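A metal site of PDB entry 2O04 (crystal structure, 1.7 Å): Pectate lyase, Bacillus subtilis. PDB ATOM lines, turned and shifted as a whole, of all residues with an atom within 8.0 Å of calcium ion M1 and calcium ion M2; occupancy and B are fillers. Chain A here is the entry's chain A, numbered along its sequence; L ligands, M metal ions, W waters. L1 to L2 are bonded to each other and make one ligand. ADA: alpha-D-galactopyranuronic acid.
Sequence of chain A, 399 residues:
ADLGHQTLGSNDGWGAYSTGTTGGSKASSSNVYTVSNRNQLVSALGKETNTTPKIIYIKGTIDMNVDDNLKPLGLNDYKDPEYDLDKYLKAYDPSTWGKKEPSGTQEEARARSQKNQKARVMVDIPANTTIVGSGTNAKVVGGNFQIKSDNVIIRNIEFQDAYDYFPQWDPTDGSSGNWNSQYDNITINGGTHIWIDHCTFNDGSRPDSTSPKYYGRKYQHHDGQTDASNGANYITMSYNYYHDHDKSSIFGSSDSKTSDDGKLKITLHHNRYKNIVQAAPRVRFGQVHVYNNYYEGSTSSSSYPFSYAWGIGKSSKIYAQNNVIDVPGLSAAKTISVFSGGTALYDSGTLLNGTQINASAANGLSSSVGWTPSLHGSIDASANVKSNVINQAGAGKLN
Calcium ion M2 is bound by OD1 of Asp 223 (2.3 Å), O6B of ADA L2 (2.5 Å), water W5 (2.5 Å), OD2 of Asp 223 (2.6 Å), water W2 (2.7 Å) and water W4 (2.9 Å).
Calcium ion M2 has six donor atoms within binding distance.
Slightly farther from calcium ion M2 lies water W6 (3.1 Å).
One residue has an atom within 4 Å of calcium ion M2: Asp 223.
The backbone NH (N) of Asp 223 is in hydrogen-bond range of the backbone carbonyl oxygen (O) of Tyr 183, 3.3 Å away.
The backbone NH (N) of Gly 224 lies close to the side-chain carboxylate (OD1) of Asp 184 (2.8 Å).
The side-chain amino group of Lys 247 lies close to the side-chain carboxylate of Asp 223, 3.8 Å away.
The backbone carbonyl oxygen (O) of Asp 227 lies within hydrogen-bond range of the backbone NH (N) of Ile 188 (2.8 Å).
The side-chain carboxylate (OD2) of Asp 184 sits close to the side-chain hydroxyl (OG1) of Thr 187 (2.7 Å).
N of Asp 227 lies within hydrogen-bond range of O of Ile 186 (3.0 Å).
The backbone NH (N) of Asp 184 is in hydrogen-bond range of the side-chain amide oxygen (OD1) of Asn 144, at 3.0 Å.
The backbone NH (N) of Ile 250 sits at hydrogen-bond distance from the side-chain carboxylate (OD1) of Asp 227 (2.9 Å).
OD2 of Asp 227 is bound to calcium ion M1, at 2.3 Å.
OD2 of Asp 223 is bound to calcium ion M1 (2.3 Å).
Calcium ion M1 is bound by the side-chain carboxylate (OD1) of Asp 184 (2.3 Å).
Water W3 binds calcium ion M1, at 2.4 Å.
Water W1 binds calcium ion M1 (2.4 Å).
Water W5 is bound to calcium ion M1 (2.5 Å).
OD2 of Asp 184 binds calcium ion M1, 2.6 Å away.
Calcium ion M1 has seven donor atoms within binding distance.
The side-chain amino group (NZ) of Lys 247 lies close to an oxygen (O6A) of ADA L2, at 2.9 Å.
Three residues have an atom within 4 Å of calcium ion M1: Asp 184, Asp 223 and Asp 227.
Along chain A the residues within 4 Å of calcium ion M1 span positions 184 to 227.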
ATOM      1  N   ASN A 144     -19.551  -4.020 -17.112  1.00  0.00           N
ATOM      2  CA  ASN A 144     -20.291  -4.764 -18.120  1.00  0.00           C
ATOM      3  C   ASN A 144     -21.744  -4.295 -18.049  1.00  0.00           C
ATOM      4  O   ASN A 144     -22.482  -4.706 -17.157  1.00  0.00           O
ATOM      5  CB  ASN A 144     -20.193  -6.267 -17.844  1.00  0.00           C
ATOM      6  CG  ASN A 144     -20.797  -7.151 -18.958  1.00  0.00           C
ATOM      7  OD1 ASN A 144     -20.457  -8.337 -19.050  1.00  0.00           O
ATOM      8  ND2 ASN A 144     -21.677  -6.598 -19.786  1.00  0.00           N
ATOM      9  N   ASN A 180     -11.680 -18.967 -20.844  1.00  0.00           N
ATOM     10  CA  ASN A 180     -12.808 -18.103 -21.167  1.00  0.00           C
ATOM     11  C   ASN A 180     -13.239 -17.251 -19.975  1.00  0.00           C
ATOM     12  O   ASN A 180     -13.269 -17.727 -18.838  1.00  0.00           O
ATOM     13  CB  ASN A 180     -13.999 -18.919 -21.662  1.00  0.00           C
ATOM     14  CG  ASN A 180     -13.733 -19.614 -22.989  1.00  0.00           C
ATOM     15  OD1 ASN A 180     -13.728 -18.984 -24.046  1.00  0.00           O
ATOM     16  ND2 ASN A 180     -13.537 -20.937 -22.944  1.00  0.00           N
ATOM     17  N   SER A 181     -13.579 -15.996 -20.254  1.00  0.00           N
ATOM     18  CA  SER A 181     -14.031 -15.057 -19.233  1.00  0.00           C
ATOM     19  C   SER A 181     -15.445 -14.561 -19.549  1.00  0.00           C
ATOM     20  O   SER A 181     -15.963 -14.802 -20.647  1.00  0.00           O
ATOM     21  CB  SER A 181     -13.045 -13.904 -19.092  1.00  0.00           C
ATOM     22  OG  SER A 181     -11.879 -14.307 -18.377  1.00  0.00           O
ATOM     23  N   GLN A 182     -16.041 -13.855 -18.601  1.00  0.00           N
ATOM     24  CA  GLN A 182     -17.490 -13.590 -18.603  1.00  0.00           C
ATOM     25  C   GLN A 182     -17.962 -12.192 -19.027  1.00  0.00           C
ATOM     26  O   GLN A 182     -19.132 -12.021 -19.377  1.00  0.00           O
ATOM     27  CB  GLN A 182     -18.079 -13.936 -17.233  1.00  0.00           C
ATOM     28  CG  GLN A 182     -18.104 -15.425 -16.943  1.00  0.00           C
ATOM     29  CD  GLN A 182     -19.044 -16.164 -17.874  1.00  0.00           C
ATOM     30  OE1 GLN A 182     -20.237 -15.870 -17.936  1.00  0.00           O
ATOM     31  NE2 GLN A 182     -18.515 -17.136 -18.603  1.00  0.00           N
ATOM     32  N   TYR A 183     -17.082 -11.200 -18.991  1.00  0.00           N
ATOM     33  CA  TYR A 183     -17.553  -9.820 -19.131  1.00  0.00           C
ATOM     34  C   TYR A 183     -17.246  -9.186 -20.479  1.00  0.00           C
ATOM     35  O   TYR A 183     -16.101  -9.233 -20.944  1.00  0.00           O
ATOM     36  CB  TYR A 183     -17.052  -8.937 -17.981  1.00  0.00           C
ATOM     37  CG  TYR A 183     -17.214  -9.628 -16.651  1.00  0.00           C
ATOM     38  CD1 TYR A 183     -18.481  -9.991 -16.194  1.00  0.00           C
ATOM     39  CD2 TYR A 183     -16.103  -9.968 -15.877  1.00  0.00           C
ATOM     40  CE1 TYR A 183     -18.640 -10.652 -14.980  1.00  0.00           C
ATOM     41  CE2 TYR A 183     -16.257 -10.636 -14.657  1.00  0.00           C
ATOM     42  CZ  TYR A 183     -17.531 -10.978 -14.223  1.00  0.00           C
ATOM     43  OH  TYR A 183     -17.697 -11.646 -13.032  1.00  0.00           O
ATOM     44  N   ASP A 184     -18.295  -8.656 -21.107  1.00  0.00           N
ATOM     45  CA  ASP A 184     -18.153  -7.756 -22.246  1.00  0.00           C
ATOM     46  C   ASP A 184     -18.256  -6.328 -21.726  1.00  0.00           C
ATOM     47  O   ASP A 184     -18.637  -6.105 -20.578  1.00  0.00           O
ATOM     48  CB  ASP A 184     -19.271  -7.971 -23.277  1.00  0.00           C
ATOM     49  CG  ASP A 184     -19.610  -9.432 -23.512  1.00  0.00           C
ATOM     50  OD1 ASP A 184     -18.687 -10.277 -23.595  1.00  0.00           O
ATOM     51  OD2 ASP A 184     -20.825  -9.717 -23.637  1.00  0.00           O
ATOM     52  N   ASN A 185     -17.938  -5.346 -22.565  1.00  0.00           N
ATOM     53  CA  ASN A 185     -18.238  -3.966 -22.202  1.00  0.00           C
ATOM     54  C   ASN A 185     -19.747  -3.730 -22.225  1.00  0.00           C
ATOM     55  O   ASN A 185     -20.306  -3.171 -21.284  1.00  0.00           O
ATOM     56  CB  ASN A 185     -17.518  -2.983 -23.119  1.00  0.00           C
ATOM     57  CG  ASN A 185     -16.044  -3.288 -23.254  1.00  0.00           C
ATOM     58  OD1 ASN A 185     -15.583  -3.717 -24.316  1.00  0.00           O
ATOM     59  ND2 ASN A 185     -15.290  -3.075 -22.179  1.00  0.00           N
ATOM     60  N   ILE A 186     -20.386  -4.169 -23.312  1.00  0.00           N
ATOM     61  CA  ILE A 186     -21.853  -4.107 -23.442  1.00  0.00           C
ATOM     62  C   ILE A 186     -22.378  -5.445 -23.955  1.00  0.00           C
ATOM     63  O   ILE A 186     -21.920  -5.946 -24.977  1.00  0.00           O
ATOM     64  CB  ILE A 186     -22.310  -2.964 -24.389  1.00  0.00           C
ATOM     65  CG1 ILE A 186     -21.851  -1.598 -23.873  1.00  0.00           C
ATOM     66  CG2 ILE A 186     -23.832  -2.986 -24.566  1.00  0.00           C
ATOM     67  CD1 ILE A 186     -22.008  -0.439 -24.862  1.00  0.00           C
ATOM     68  N   THR A 187     -23.345  -6.016 -23.229  1.00  0.00           N
ATOM     69  CA  THR A 187     -24.042  -7.228 -23.662  1.00  0.00           C
ATOM     70  C   THR A 187     -25.500  -6.911 -23.912  1.00  0.00           C
ATOM     71  O   THR A 187     -26.218  -6.494 -22.999  1.00  0.00           O
ATOM     72  CB  THR A 187     -23.993  -8.325 -22.584  1.00  0.00           C
ATOM     73  OG1 THR A 187     -22.651  -8.519 -22.132  1.00  0.00           O
ATOM     74  CG2 THR A 187     -24.547  -9.635 -23.128  1.00  0.00           C
ATOM     75  N   ILE A 188     -25.941  -7.100 -25.146  1.00  0.00           N
ATOM     76  CA  ILE A 188     -27.351  -6.922 -25.480  1.00  0.00           C
ATOM     77  C   ILE A 188     -27.992  -8.303 -25.421  1.00  0.00           C
ATOM     78  O   ILE A 188     -27.840  -9.117 -26.340  1.00  0.00           O
ATOM     79  CB  ILE A 188     -27.553  -6.267 -26.854  1.00  0.00           C
ATOM     80  CG1 ILE A 188     -26.812  -4.920 -26.936  1.00  0.00           C
ATOM     81  CG2 ILE A 188     -29.027  -6.083 -27.138  1.00  0.00           C
ATOM     82  CD1 ILE A 188     -26.661  -4.383 -28.355  1.00  0.00           C
ATOM     83  N   HIS A 222     -10.599 -11.336 -20.713  1.00  0.00           N
ATOM     84  CA  HIS A 222     -11.642 -10.579 -21.420  1.00  0.00           C
ATOM     85  C   HIS A 222     -12.560 -11.483 -22.211  1.00  0.00           C
ATOM     86  O   HIS A 222     -12.194 -12.608 -22.556  1.00  0.00           O
ATOM     87  CB  HIS A 222     -11.006  -9.574 -22.385  1.00  0.00           C
ATOM     88  CG  HIS A 222     -10.071  -8.612 -21.723  1.00  0.00           C
ATOM     89  ND1 HIS A 222      -8.729  -8.569 -22.012  1.00  0.00           N
ATOM     90  CD2 HIS A 222     -10.289  -7.664 -20.770  1.00  0.00           C
ATOM     91  CE1 HIS A 222      -8.154  -7.637 -21.272  1.00  0.00           C
ATOM     92  NE2 HIS A 222      -9.080  -7.077 -20.513  1.00  0.00           N
ATOM     93  N   ASP A 223     -13.746 -10.979 -22.515  1.00  0.00           N
ATOM     94  CA  ASP A 223     -14.641 -11.641 -23.439  1.00  0.00           C
ATOM     95  C   ASP A 223     -14.893 -10.691 -24.611  1.00  0.00           C
ATOM     96  O   ASP A 223     -13.954 -10.276 -25.295  1.00  0.00           O
ATOM     97  CB  ASP A 223     -15.932 -12.043 -22.742  1.00  0.00           C
ATOM     98  CG  ASP A 223     -16.710 -13.095 -23.500  1.00  0.00           C
ATOM     99  OD1 ASP A 223     -16.134 -14.178 -23.806  1.00  0.00           O
ATOM    100  OD2 ASP A 223     -17.901 -12.861 -23.783  1.00  0.00           O
ATOM    101  N   GLY A 224     -16.149 -10.303 -24.815  1.00  0.00           N
ATOM    102  CA  GLY A 224     -16.521  -9.447 -25.927  1.00  0.00           C
ATOM    103  C   GLY A 224     -16.451  -7.966 -25.631  1.00  0.00           C
ATOM    104  O   GLY A 224     -16.142  -7.535 -24.522  1.00  0.00           O
ATOM    105  N   GLN A 225     -16.743  -7.174 -26.655  1.00  0.00           N
ATOM    106  CA  GLN A 225     -16.831  -5.734 -26.519  1.00  0.00           C
ATOM    107  C   GLN A 225     -18.293  -5.319 -26.593  1.00  0.00           C
ATOM    108  O   GLN A 225     -18.848  -4.818 -25.618  1.00  0.00           O
ATOM    109  CB  GLN A 225     -15.979  -5.045 -27.578  1.00  0.00           C
ATOM    110  CG  GLN A 225     -14.502  -5.368 -27.412  1.00  0.00           C
ATOM    111  CD  GLN A 225     -13.610  -4.652 -28.412  1.00  0.00           C
ATOM    112  OE1 GLN A 225     -13.702  -4.883 -29.620  1.00  0.00           O
ATOM    113  NE2 GLN A 225     -12.718  -3.815 -27.903  1.00  0.00           N
ATOM    114  N   THR A 226     -18.905  -5.538 -27.749  1.00  0.00           N
ATOM    115  CA  THR A 226     -20.343  -5.321 -27.904  1.00  0.00           C
ATOM    116  C   THR A 226     -20.979  -6.580 -28.478  1.00  0.00           C
ATOM    117  O   THR A 226     -20.932  -6.810 -29.697  1.00  0.00           O
ATOM    118  CB  THR A 226     -20.660  -4.113 -28.815  1.00  0.00           C
ATOM    119  OG1 THR A 226     -19.953  -4.250 -30.048  1.00  0.00           O
ATOM    120  CG2 THR A 226     -20.262  -2.807 -28.129  1.00  0.00           C
ATOM    121  N   ASP A 227     -21.570  -7.386 -27.610  1.00  0.00           N
ATOM    122  CA  ASP A 227     -22.175  -8.648 -28.002  1.00  0.00           C
ATOM    123  C   ASP A 227     -23.703  -8.545 -28.019  1.00  0.00           C
ATOM    124  O   ASP A 227     -24.280  -7.722 -27.316  1.00  0.00           O
ATOM    125  CB  ASP A 227     -21.750  -9.763 -27.044  1.00  0.00           C
ATOM    126  CG  ASP A 227     -20.302 -10.174 -27.225  1.00  0.00           C
ATOM    127  OD1 ASP A 227     -19.671  -9.833 -28.251  1.00  0.00           O
ATOM    128  OD2 ASP A 227     -19.787 -10.878 -26.326  1.00  0.00           O
ATOM    129  N   ALA A 228     -24.337  -9.377 -28.838  1.00  0.00           N
ATOM    130  CA  ALA A 228     -25.796  -9.416 -28.900  1.00  0.00           C
ATOM    131  C   ALA A 228     -26.257 -10.865 -28.987  1.00  0.00           C
ATOM    132  O   ALA A 228     -25.732 -11.645 -29.776  1.00  0.00           O
ATOM    133  CB  ALA A 228     -26.312  -8.608 -30.083  1.00  0.00           C
ATOM    134  N   SER A 229     -27.231 -11.219 -28.147  1.00  0.00           N
ATOM    135  CA  SER A 229     -27.703 -12.601 -28.051  1.00  0.00           C
ATOM    136  C   SER A 229     -29.180 -12.666 -27.687  1.00  0.00           C
ATOM    137  O   SER A 229     -29.788 -11.640 -27.372  1.00  0.00           O
ATOM    138  CB  SER A 229     -26.883 -13.363 -27.009  1.00  0.00           C
ATOM    139  OG  SER A 229     -27.345 -14.702 -26.901  1.00  0.00           O
ATOM    140  N   LYS A 247     -11.743 -10.811 -29.077  1.00  0.00           N
ATOM    141  CA  LYS A 247     -13.060 -11.096 -29.672  1.00  0.00           C
ATOM    142  C   LYS A 247     -13.993  -9.899 -29.519  1.00  0.00           C
ATOM    143  O   LYS A 247     -14.445  -9.590 -28.419  1.00  0.00           O
ATOM    144  CB  LYS A 247     -13.674 -12.338 -29.015  1.00  0.00           C
ATOM    145  CG  LYS A 247     -12.816 -13.601 -29.072  1.00  0.00           C
ATOM    146  CD  LYS A 247     -13.318 -14.697 -28.125  1.00  0.00           C
ATOM    147  CE  LYS A 247     -13.007 -14.370 -26.658  1.00  0.00           C
ATOM    148  NZ  LYS A 247     -13.112 -15.557 -25.737  1.00  0.00           N
ATOM    149  N   SER A 248     -14.297  -9.212 -30.619  1.00  0.00           N
ATOM    150  CA  SER A 248     -15.015  -7.943 -30.526  1.00  0.00           C
ATOM    151  C   SER A 248     -16.539  -8.041 -30.378  1.00  0.00           C
ATOM    152  O   SER A 248     -17.113  -7.561 -29.395  1.00  0.00           O
ATOM    153  CB  SER A 248     -14.685  -7.034 -31.711  1.00  0.00           C
ATOM    154  OG  SER A 248     -15.449  -5.842 -31.626  1.00  0.00           O
ATOM    155  N   ILE A 250     -19.864 -10.515 -31.098  1.00  0.00           N
ATOM    156  CA  ILE A 250     -20.536 -11.764 -31.429  1.00  0.00           C
ATOM    157  C   ILE A 250     -22.046 -11.556 -31.395  1.00  0.00           C
ATOM    158  O   ILE A 250     -22.619 -11.233 -30.339  1.00  0.00           O
ATOM    159  CB  ILE A 250     -20.059 -12.935 -30.520  1.00  0.00           C
ATOM    160  CG1 ILE A 250     -18.568 -13.217 -30.815  1.00  0.00           C
ATOM    161  CG2 ILE A 250     -20.917 -14.200 -30.759  1.00  0.00           C
ATOM    162  CD1 ILE A 250     -17.904 -14.232 -29.920  1.00  0.00           C
ATOM    163  N   SER A 253     -25.347 -16.179 -30.158  1.00  0.00           N
ATOM    164  CA  SER A 253     -24.397 -16.860 -29.299  1.00  0.00           C
ATOM    165  C   SER A 253     -24.324 -18.370 -29.498  1.00  0.00           C
ATOM    166  O   SER A 253     -23.433 -19.026 -28.957  1.00  0.00           O
ATOM    167  CB  SER A 253     -24.723 -16.556 -27.837  1.00  0.00           C
ATOM    168  OG  SER A 253     -25.921 -17.208 -27.457  1.00  0.00           O
HETATM  169  C1  ADA L   1     -12.501 -18.714 -31.478  1.00  0.00           C
HETATM  170  C2  ADA L   1     -12.778 -19.173 -30.049  1.00  0.00           C
HETATM  171  C3  ADA L   1     -13.647 -20.428 -30.031  1.00  0.00           C
HETATM  172  C4  ADA L   1     -14.911 -20.264 -30.888  1.00  0.00           C
HETATM  173  C5  ADA L   1     -14.576 -19.713 -32.282  1.00  0.00           C
HETATM  174  C6  ADA L   1     -15.825 -19.359 -33.045  1.00  0.00           C
HETATM  175  O1  ADA L   1     -11.653 -19.657 -32.152  1.00  0.00           O
HETATM  176  O2  ADA L   1     -11.537 -19.448 -29.383  1.00  0.00           O
HETATM  177  O3  ADA L   1     -13.984 -20.759 -28.680  1.00  0.00           O
HETATM  178  O4  ADA L   1     -15.848 -19.384 -30.239  1.00  0.00           O
HETATM  179  O5  ADA L   1     -13.743 -18.545 -32.192  1.00  0.00           O
HETATM  180  O6B ADA L   1     -16.649 -20.255 -33.330  1.00  0.00           O
HETATM  181  O6A ADA L   1     -15.998 -18.159 -33.380  1.00  0.00           O
HETATM  182  C1  ADA L   2     -16.898 -19.795 -29.350  1.00  0.00           C
HETATM  183  C2  ADA L   2     -18.363 -19.561 -29.728  1.00  0.00           C
HETATM  184  C3  ADA L   2     -18.697 -18.069 -29.743  1.00  0.00           C
HETATM  185  C4  ADA L   2     -18.215 -17.393 -28.454  1.00  0.00           C
HETATM  186  C5  ADA L   2     -16.716 -17.645 -28.308  1.00  0.00           C
HETATM  187  C6  ADA L   2     -16.086 -16.910 -27.152  1.00  0.00           C
HETATM  188  O2  ADA L   2     -18.595 -20.130 -31.022  1.00  0.00           O
HETATM  189  O3  ADA L   2     -20.103 -17.858 -29.937  1.00  0.00           O
HETATM  190  O4  ADA L   2     -18.923 -17.906 -27.323  1.00  0.00           O
HETATM  191  O5  ADA L   2     -16.514 -19.061 -28.183  1.00  0.00           O
HETATM  192  O6B ADA L   2     -16.551 -15.799 -26.813  1.00  0.00           O
HETATM  193  O6A ADA L   2     -15.100 -17.425 -26.563  1.00  0.00           O
HETATM  194 CA    CA M   1     -20.007 -12.045 -24.338  1.00  0.00          CA
HETATM  195 CA    CA M   2     -17.923 -15.279 -24.802  1.00  0.00          CA
HETATM  196 CA    CA M   3     -14.545 -19.668 -26.376  1.00  0.00          CA
HETATM  197  O   HOH W   1     -20.431 -12.503 -22.013  1.00  0.00           O
HETATM  198  O   HOH W   2     -16.291 -16.850 -23.399  1.00  0.00           O
HETATM  199  O   HOH W   3     -22.326 -12.484 -24.761  1.00  0.00           O
HETATM  200  O   HOH W   4     -18.256 -15.695 -21.959  1.00  0.00           O
HETATM  201  O   HOH W   5     -19.479 -13.760 -26.019  1.00  0.00           O
HETATM  202  O   HOH W   6     -16.905 -13.134 -26.815  1.00  0.00           O
